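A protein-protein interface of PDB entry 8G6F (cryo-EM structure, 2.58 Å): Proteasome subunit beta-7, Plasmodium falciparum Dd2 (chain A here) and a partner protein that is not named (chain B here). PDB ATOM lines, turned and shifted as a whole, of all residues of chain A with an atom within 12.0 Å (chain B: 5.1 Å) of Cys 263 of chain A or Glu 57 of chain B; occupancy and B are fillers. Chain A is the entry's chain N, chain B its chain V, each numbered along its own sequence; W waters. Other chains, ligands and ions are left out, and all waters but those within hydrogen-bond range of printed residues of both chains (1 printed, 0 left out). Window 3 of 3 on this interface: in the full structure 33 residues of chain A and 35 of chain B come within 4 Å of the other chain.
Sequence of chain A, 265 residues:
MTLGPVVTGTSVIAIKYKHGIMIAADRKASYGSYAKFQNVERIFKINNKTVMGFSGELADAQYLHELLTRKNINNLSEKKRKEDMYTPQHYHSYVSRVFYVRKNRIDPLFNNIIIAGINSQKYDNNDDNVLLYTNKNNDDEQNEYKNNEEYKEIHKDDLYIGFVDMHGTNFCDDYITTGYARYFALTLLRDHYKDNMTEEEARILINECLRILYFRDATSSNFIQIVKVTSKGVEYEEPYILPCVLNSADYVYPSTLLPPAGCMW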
ATOM      1  N   PRO A 254     -14.776   6.961   6.786  1.00  0.00           N
ATOM      2  CA  PRO A 254     -14.244   5.676   7.257  1.00  0.00           C
ATOM      3  C   PRO A 254     -13.809   4.775   6.112  1.00  0.00           C
ATOM      4  O   PRO A 254     -14.402   4.768   5.033  1.00  0.00           O
ATOM      5  CB  PRO A 254     -15.420   5.064   8.028  1.00  0.00           C
ATOM      6  CG  PRO A 254     -16.260   6.206   8.412  1.00  0.00           C
ATOM      7  CD  PRO A 254     -16.117   7.226   7.333  1.00  0.00           C
ATOM      8  N   SER A 255     -12.749   4.006   6.365  1.00  0.00           N
ATOM      9  CA  SER A 255     -12.215   3.119   5.339  1.00  0.00           C
ATOM     10  C   SER A 255     -13.146   1.948   5.068  1.00  0.00           C
ATOM     11  O   SER A 255     -13.180   1.435   3.946  1.00  0.00           O
ATOM     12  CB  SER A 255     -10.838   2.607   5.752  1.00  0.00           C
ATOM     13  OG  SER A 255     -10.047   3.652   6.278  1.00  0.00           O
ATOM     14  N   THR A 256     -13.898   1.507   6.078  1.00  0.00           N
ATOM     15  CA  THR A 256     -14.825   0.398   5.906  1.00  0.00           C
ATOM     16  C   THR A 256     -16.002   0.746   5.009  1.00  0.00           C
ATOM     17  O   THR A 256     -16.717  -0.165   4.580  1.00  0.00           O
ATOM     18  CB  THR A 256     -15.350  -0.070   7.263  1.00  0.00           C
ATOM     19  OG1 THR A 256     -15.589   1.063   8.105  1.00  0.00           O
ATOM     20  CG2 THR A 256     -14.351  -0.994   7.930  1.00  0.00           C
ATOM     21  N   LEU A 257     -16.234   2.024   4.731  1.00  0.00           N
ATOM     22  CA  LEU A 257     -17.288   2.432   3.816  1.00  0.00           C
ATOM     23  C   LEU A 257     -16.826   2.473   2.368  1.00  0.00           C
ATOM     24  O   LEU A 257     -17.652   2.686   1.476  1.00  0.00           O
ATOM     25  CB  LEU A 257     -17.834   3.801   4.219  1.00  0.00           C
ATOM     26  CG  LEU A 257     -18.818   3.782   5.388  1.00  0.00           C
ATOM     27  CD1 LEU A 257     -18.955   5.159   5.986  1.00  0.00           C
ATOM     28  CD2 LEU A 257     -20.167   3.258   4.949  1.00  0.00           C
ATOM     29  N   LEU A 258     -15.541   2.285   2.119  1.00  0.00           N
ATOM     30  CA  LEU A 258     -15.011   2.121   0.779  1.00  0.00           C
ATOM     31  C   LEU A 258     -15.135   0.668   0.345  1.00  0.00           C
ATOM     32  O   LEU A 258     -15.237  -0.231   1.182  1.00  0.00           O
ATOM     33  CB  LEU A 258     -13.551   2.559   0.738  1.00  0.00           C
ATOM     34  CG  LEU A 258     -13.290   4.029   1.063  1.00  0.00           C
ATOM     35  CD1 LEU A 258     -11.800   4.303   1.114  1.00  0.00           C
ATOM     36  CD2 LEU A 258     -13.965   4.935   0.054  1.00  0.00           C
ATOM     37  N   PRO A 259     -15.136   0.397  -0.958  1.00  0.00           N
ATOM     38  CA  PRO A 259     -15.278  -0.985  -1.426  1.00  0.00           C
ATOM     39  C   PRO A 259     -14.199  -1.877  -0.840  1.00  0.00           C
ATOM     40  O   PRO A 259     -13.026  -1.482  -0.782  1.00  0.00           O
ATOM     41  CB  PRO A 259     -15.131  -0.853  -2.947  1.00  0.00           C
ATOM     42  CG  PRO A 259     -15.606   0.510  -3.234  1.00  0.00           C
ATOM     43  CD  PRO A 259     -15.142   1.350  -2.081  1.00  0.00           C
ATOM     44  N   PRO A 260     -14.544  -3.091  -0.396  1.00  0.00           N
ATOM     45  CA  PRO A 260     -13.534  -3.952   0.236  1.00  0.00           C
ATOM     46  C   PRO A 260     -12.557  -4.587  -0.737  1.00  0.00           C
ATOM     47  O   PRO A 260     -11.601  -5.233  -0.287  1.00  0.00           O
ATOM     48  CB  PRO A 260     -14.376  -5.033   0.936  1.00  0.00           C
ATOM     49  CG  PRO A 260     -15.799  -4.592   0.818  1.00  0.00           C
ATOM     50  CD  PRO A 260     -15.865  -3.736  -0.393  1.00  0.00           C
ATOM     51  N   ALA A 261     -12.760  -4.435  -2.042  1.00  0.00           N
ATOM     52  CA  ALA A 261     -11.895  -5.032  -3.046  1.00  0.00           C
ATOM     53  C   ALA A 261     -10.999  -3.968  -3.664  1.00  0.00           C
ATOM     54  O   ALA A 261     -11.392  -2.804  -3.784  1.00  0.00           O
ATOM     55  CB  ALA A 261     -12.720  -5.716  -4.136  1.00  0.00           C
ATOM     56  N   GLY A 262      -9.793  -4.369  -4.046  1.00  0.00           N
ATOM     57  CA  GLY A 262      -8.892  -3.476  -4.745  1.00  0.00           C
ATOM     58  C   GLY A 262      -7.862  -2.827  -3.847  1.00  0.00           C
ATOM     59  O   GLY A 262      -7.450  -3.404  -2.838  1.00  0.00           O
ATOM     60  N   CYS A 263      -7.429  -1.619  -4.214  1.00  0.00           N
ATOM     61  CA  CYS A 263      -6.473  -0.837  -3.430  1.00  0.00           C
ATOM     62  C   CYS A 263      -7.104   0.530  -3.203  1.00  0.00           C
ATOM     63  O   CYS A 263      -6.838   1.478  -3.942  1.00  0.00           O
ATOM     64  CB  CYS A 263      -5.130  -0.728  -4.149  1.00  0.00           C
ATOM     65  SG  CYS A 263      -4.463  -2.288  -4.746  1.00  0.00           S
ATOM     66  N   MET A 264      -7.930   0.633  -2.162  1.00  0.00           N
ATOM     67  CA  MET A 264      -8.644   1.869  -1.883  1.00  0.00           C
ATOM     68  C   MET A 264      -7.944   2.744  -0.856  1.00  0.00           C
ATOM     69  O   MET A 264      -8.221   3.947  -0.804  1.00  0.00           O
ATOM     70  CB  MET A 264     -10.067   1.562  -1.401  1.00  0.00           C
ATOM     71  CG  MET A 264     -11.028   1.217  -2.531  1.00  0.00           C
ATOM     72  SD  MET A 264     -11.274   2.586  -3.677  1.00  0.00           S
ATOM     73  CE  MET A 264     -12.510   1.905  -4.776  1.00  0.00           C
ATOM     74  N   TRP A 265      -7.053   2.176  -0.052  1.00  0.00           N
ATOM     75  CA  TRP A 265      -6.263   2.943   0.901  1.00  0.00           C
ATOM     76  C   TRP A 265      -5.739   4.235   0.277  1.00  0.00           C
ATOM     77  O   TRP A 265      -4.836   4.878   0.813  1.00  0.00           O
ATOM     78  CB  TRP A 265      -5.092   2.103   1.415  1.00  0.00           C
ATOM     79  CG  TRP A 265      -4.400   1.324   0.339  1.00  0.00           C
ATOM     80  CD1 TRP A 265      -3.687   1.826  -0.704  1.00  0.00           C
ATOM     81  CD2 TRP A 265      -4.363  -0.101   0.202  1.00  0.00           C
ATOM     82  NE1 TRP A 265      -3.209   0.805  -1.485  1.00  0.00           N
ATOM     83  CE2 TRP A 265      -3.607  -0.388  -0.948  1.00  0.00           C
ATOM     84  CE3 TRP A 265      -4.895  -1.161   0.940  1.00  0.00           C
ATOM     85  CZ2 TRP A 265      -3.370  -1.689  -1.377  1.00  0.00           C
ATOM     86  CZ3 TRP A 265      -4.657  -2.450   0.512  1.00  0.00           C
ATOM     87  CH2 TRP A 265      -3.900  -2.704  -0.634  1.00  0.00           C
ATOM     88  N   SER B  52       4.290  -2.748   1.785  1.00  0.00           N
ATOM     89  CA  SER B  52       3.155  -3.182   2.586  1.00  0.00           C
ATOM     90  C   SER B  52       1.885  -3.264   1.748  1.00  0.00           C
ATOM     91  O   SER B  52       1.111  -4.213   1.892  1.00  0.00           O
ATOM     92  CB  SER B  52       2.961  -2.255   3.784  1.00  0.00           C
ATOM     93  OG  SER B  52       3.087  -0.897   3.425  1.00  0.00           O
ATOM     94  N   GLN B  53       1.658  -2.301   0.854  1.00  0.00           N
ATOM     95  CA  GLN B  53       0.442  -2.310   0.048  1.00  0.00           C
ATOM     96  C   GLN B  53       0.405  -3.506  -0.894  1.00  0.00           C
ATOM     97  O   GLN B  53      -0.624  -4.180  -1.016  1.00  0.00           O
ATOM     98  CB  GLN B  53       0.336  -1.008  -0.741  1.00  0.00           C
ATOM     99  CG  GLN B  53      -0.138   0.170   0.078  1.00  0.00           C
ATOM    100  CD  GLN B  53      -0.027   1.473  -0.671  1.00  0.00           C
ATOM    101  OE1 GLN B  53       0.069   1.488  -1.893  1.00  0.00           O
ATOM    102  NE2 GLN B  53      -0.043   2.577   0.056  1.00  0.00           N
ATOM    103  N   LYS B  54       1.514  -3.788  -1.580  1.00  0.00           N
ATOM    104  CA  LYS B  54       1.515  -4.913  -2.506  1.00  0.00           C
ATOM    105  C   LYS B  54       1.396  -6.237  -1.764  1.00  0.00           C
ATOM    106  O   LYS B  54       0.686  -7.152  -2.214  1.00  0.00           O
ATOM    107  CB  LYS B  54       2.774  -4.878  -3.367  1.00  0.00           C
ATOM    108  CG  LYS B  54       2.868  -3.642  -4.243  1.00  0.00           C
ATOM    109  CD  LYS B  54       1.726  -3.548  -5.233  1.00  0.00           C
ATOM    110  CE  LYS B  54       0.755  -2.450  -4.851  1.00  0.00           C
ATOM    111  NZ  LYS B  54      -0.602  -2.686  -5.400  1.00  0.00           N
ATOM    112  N   ILE B  55       2.057  -6.354  -0.612  1.00  0.00           N
ATOM    113  CA  ILE B  55       1.913  -7.561   0.192  1.00  0.00           C
ATOM    114  C   ILE B  55       0.461  -7.744   0.607  1.00  0.00           C
ATOM    115  O   ILE B  55      -0.089  -8.846   0.523  1.00  0.00           O
ATOM    116  CB  ILE B  55       2.849  -7.507   1.413  1.00  0.00           C
ATOM    117  CG1 ILE B  55       4.301  -7.731   0.990  1.00  0.00           C
ATOM    118  CG2 ILE B  55       2.433  -8.536   2.451  1.00  0.00           C
ATOM    119  CD1 ILE B  55       4.528  -8.988   0.184  1.00  0.00           C
ATOM    120  N   ILE B  56      -0.182  -6.668   1.058  1.00  0.00           N
ATOM    121  CA  ILE B  56      -1.553  -6.780   1.537  1.00  0.00           C
ATOM    122  C   ILE B  56      -2.493  -7.138   0.394  1.00  0.00           C
ATOM    123  O   ILE B  56      -3.460  -7.879   0.587  1.00  0.00           O
ATOM    124  CB  ILE B  56      -1.976  -5.479   2.246  1.00  0.00           C
ATOM    125  CG1 ILE B  56      -1.243  -5.323   3.583  1.00  0.00           C
ATOM    126  CG2 ILE B  56      -3.473  -5.450   2.472  1.00  0.00           C
ATOM    127  CD1 ILE B  56      -1.160  -6.579   4.424  1.00  0.00           C
ATOM    128  N   GLU B  57      -2.231  -6.632  -0.808  1.00  0.00           N
ATOM    129  CA  GLU B  57      -3.049  -7.024  -1.951  1.00  0.00           C
ATOM    130  C   GLU B  57      -2.923  -8.521  -2.228  1.00  0.00           C
ATOM    131  O   GLU B  57      -3.930  -9.225  -2.411  1.00  0.00           O
ATOM    132  CB  GLU B  57      -2.649  -6.210  -3.179  1.00  0.00           C
ATOM    133  CG  GLU B  57      -3.583  -6.389  -4.354  1.00  0.00           C
ATOM    134  CD  GLU B  57      -3.148  -5.604  -5.570  1.00  0.00           C
ATOM    135  OE1 GLU B  57      -1.943  -5.301  -5.685  1.00  0.00           O
ATOM    136  OE2 GLU B  57      -4.015  -5.292  -6.413  1.00  0.00           O
ATOM    137  N   ILE B  58      -1.690  -9.031  -2.238  1.00  0.00           N
ATOM    138  CA  ILE B  58      -1.495 -10.463  -2.448  1.00  0.00           C
ATOM    139  C   ILE B  58      -2.212 -11.264  -1.366  1.00  0.00           C
ATOM    140  O   ILE B  58      -2.846 -12.288  -1.644  1.00  0.00           O
ATOM    141  CB  ILE B  58       0.005 -10.799  -2.491  1.00  0.00           C
ATOM    142  CG1 ILE B  58       0.639 -10.252  -3.766  1.00  0.00           C
ATOM    143  CG2 ILE B  58       0.213 -12.294  -2.415  1.00  0.00           C
ATOM    144  CD1 ILE B  58       2.133 -10.112  -3.684  1.00  0.00           C
ATOM    145  N   ILE B  59      -2.108 -10.819  -0.114  1.00  0.00           N
ATOM    146  CA  ILE B  59      -2.696 -11.566   0.992  1.00  0.00           C
ATOM    147  C   ILE B  59      -4.215 -11.524   0.937  1.00  0.00           C
ATOM    148  O   ILE B  59      -4.876 -12.489   1.323  1.00  0.00           O
ATOM    149  CB  ILE B  59      -2.162 -11.033   2.335  1.00  0.00           C
ATOM    150  CG1 ILE B  59      -0.653 -11.276   2.461  1.00  0.00           C
ATOM    151  CG2 ILE B  59      -2.891 -11.687   3.496  1.00  0.00           C
ATOM    152  CD1 ILE B  59      -0.195 -12.672   2.091  1.00  0.00           C
ATOM    153  N   LYS B  60      -4.800 -10.415   0.488  1.00  0.00           N
ATOM    154  CA  LYS B  60      -6.247 -10.368   0.304  1.00  0.00           C
ATOM    155  C   LYS B  60      -6.692 -11.363  -0.758  1.00  0.00           C
ATOM    156  O   LYS B  60      -7.715 -12.042  -0.602  1.00  0.00           O
ATOM    157  CB  LYS B  60      -6.677  -8.954  -0.076  1.00  0.00           C
ATOM    158  CG  LYS B  60      -6.832  -8.020   1.103  1.00  0.00           C
ATOM    159  CD  LYS B  60      -6.741  -6.569   0.678  1.00  0.00           C
ATOM    160  CE  LYS B  60      -7.797  -6.224  -0.349  1.00  0.00           C
ATOM    161  NZ  LYS B  60      -8.393  -4.884  -0.124  1.00  0.00           N
ATOM    162  N   HIS B  61      -5.932 -11.462  -1.848  1.00  0.00           N
ATOM    163  CA  HIS B  61      -6.224 -12.461  -2.875  1.00  0.00           C
ATOM    164  C   HIS B  61      -6.149 -13.879  -2.300  1.00  0.00           C
ATOM    165  O   HIS B  61      -7.054 -14.708  -2.505  1.00  0.00           O
ATOM    166  CB  HIS B  61      -5.247 -12.238  -4.035  1.00  0.00           C
ATOM    167  CG  HIS B  61      -4.988 -13.438  -4.884  1.00  0.00           C
ATOM    168  ND1 HIS B  61      -5.926 -13.959  -5.747  1.00  0.00           N
ATOM    169  CD2 HIS B  61      -3.872 -14.185  -5.048  1.00  0.00           C
ATOM    170  CE1 HIS B  61      -5.410 -14.994  -6.383  1.00  0.00           C
ATOM    171  NE2 HIS B  61      -4.165 -15.153  -5.976  1.00  0.00           N
HETATM  172  O   HOH W   1      -1.061   0.257  -3.876  1.00  0.00           O
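O of Pro 260 of chain A sits at hydrogen-bond distance from NZ of Lys 60 of chain B, 3.2 Å away.
O of Gly 262 of chain A lies within hydrogen-bond range of NZ of Lys 60 of chain B.
The side-chain sulfur (SG) of Cys 263 of chain A lies within hydrogen-bond range of the side-chain carboxylate (OE2) of Glu 57 of chain B, at 3.5 Å.
NE1 of Trp 265 of chain A lies close to OE1 of Gln 53 of chain B (3.4 Å).
The side-chain carboxylate (OE1) of Glu 57 of chain B is in salt-bridge range of the side-chain amino group (NZ) of Lys 54 of chain B (3.0 Å).
Among the printed residues, merely in contact across the chains: Trp 265 of chain A with Ile 56 of chain B (3.8 Å) and Cys 263 of chain A with Lys 54 of chain B (3.9 Å).
Printed residues of chain B within 4 Å of Pro 260 of chain A: Lys 60 (3.2 Å).
Printed residues of chain B within 4 Å of Gly 262 of chain A: Lys 60.
Met 264 of chain A touches none of the printed residues of chain B.
Of the printed residues of chain B, Trp 265 of chain A touches Gln 53 and Ile 56.
Lys 54 of chain B touches just one residue of chain A: Cys 263 (3.9 Å).
No residue of chain A comes within 4 Å of Ile 55 of chain B.
Ile 56 of chain B touches one residue of chain A.
Glu 57 of chain B touches one residue of chain A.
No residue of chain A comes within 4 Å of Ile 58 of chain B.
No residue of chain A comes within 4 Å of Ile 59 of chain B.
No residue of chain A comes within 4 Å of His 61 of chain B.
The nearest printed residue of chain B that does not touch Cys 263 of chain A is Lys 60 of chain B (5.3 Å).
The nearest printed residue of chain B that does not touch Trp 265 of chain A is Glu 57 of chain B (4.3 Å).
Of the 10 printed residues of chain B, 5 touch a printed residue of chain A.
Printed residues of chain B that touch a printed residue of chain A: Gln 53, Lys 54, Ile 56, Glu 57 and Lys 60.
Of the 12 printed residues of chain A, 4 touch a printed residue of chain B.
Printed residues of chain A that touch a printed residue of chain B: Pro 260, Gly 262, Cys 263 and Trp 265.
Among the printed residues, no Asp or Glu carboxylate lies within 4 Å of a Lys or Arg side-chain nitrogen of the other chain.
Water W1 lies within hydrogen-bond range of the side-chain amide oxygen (OE1) of Gln 53 of chain B, the indole nitrogen (NE1) of Trp 265 of chain A and the side-chain amino group (NZ) of Lys 54 of chain B.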
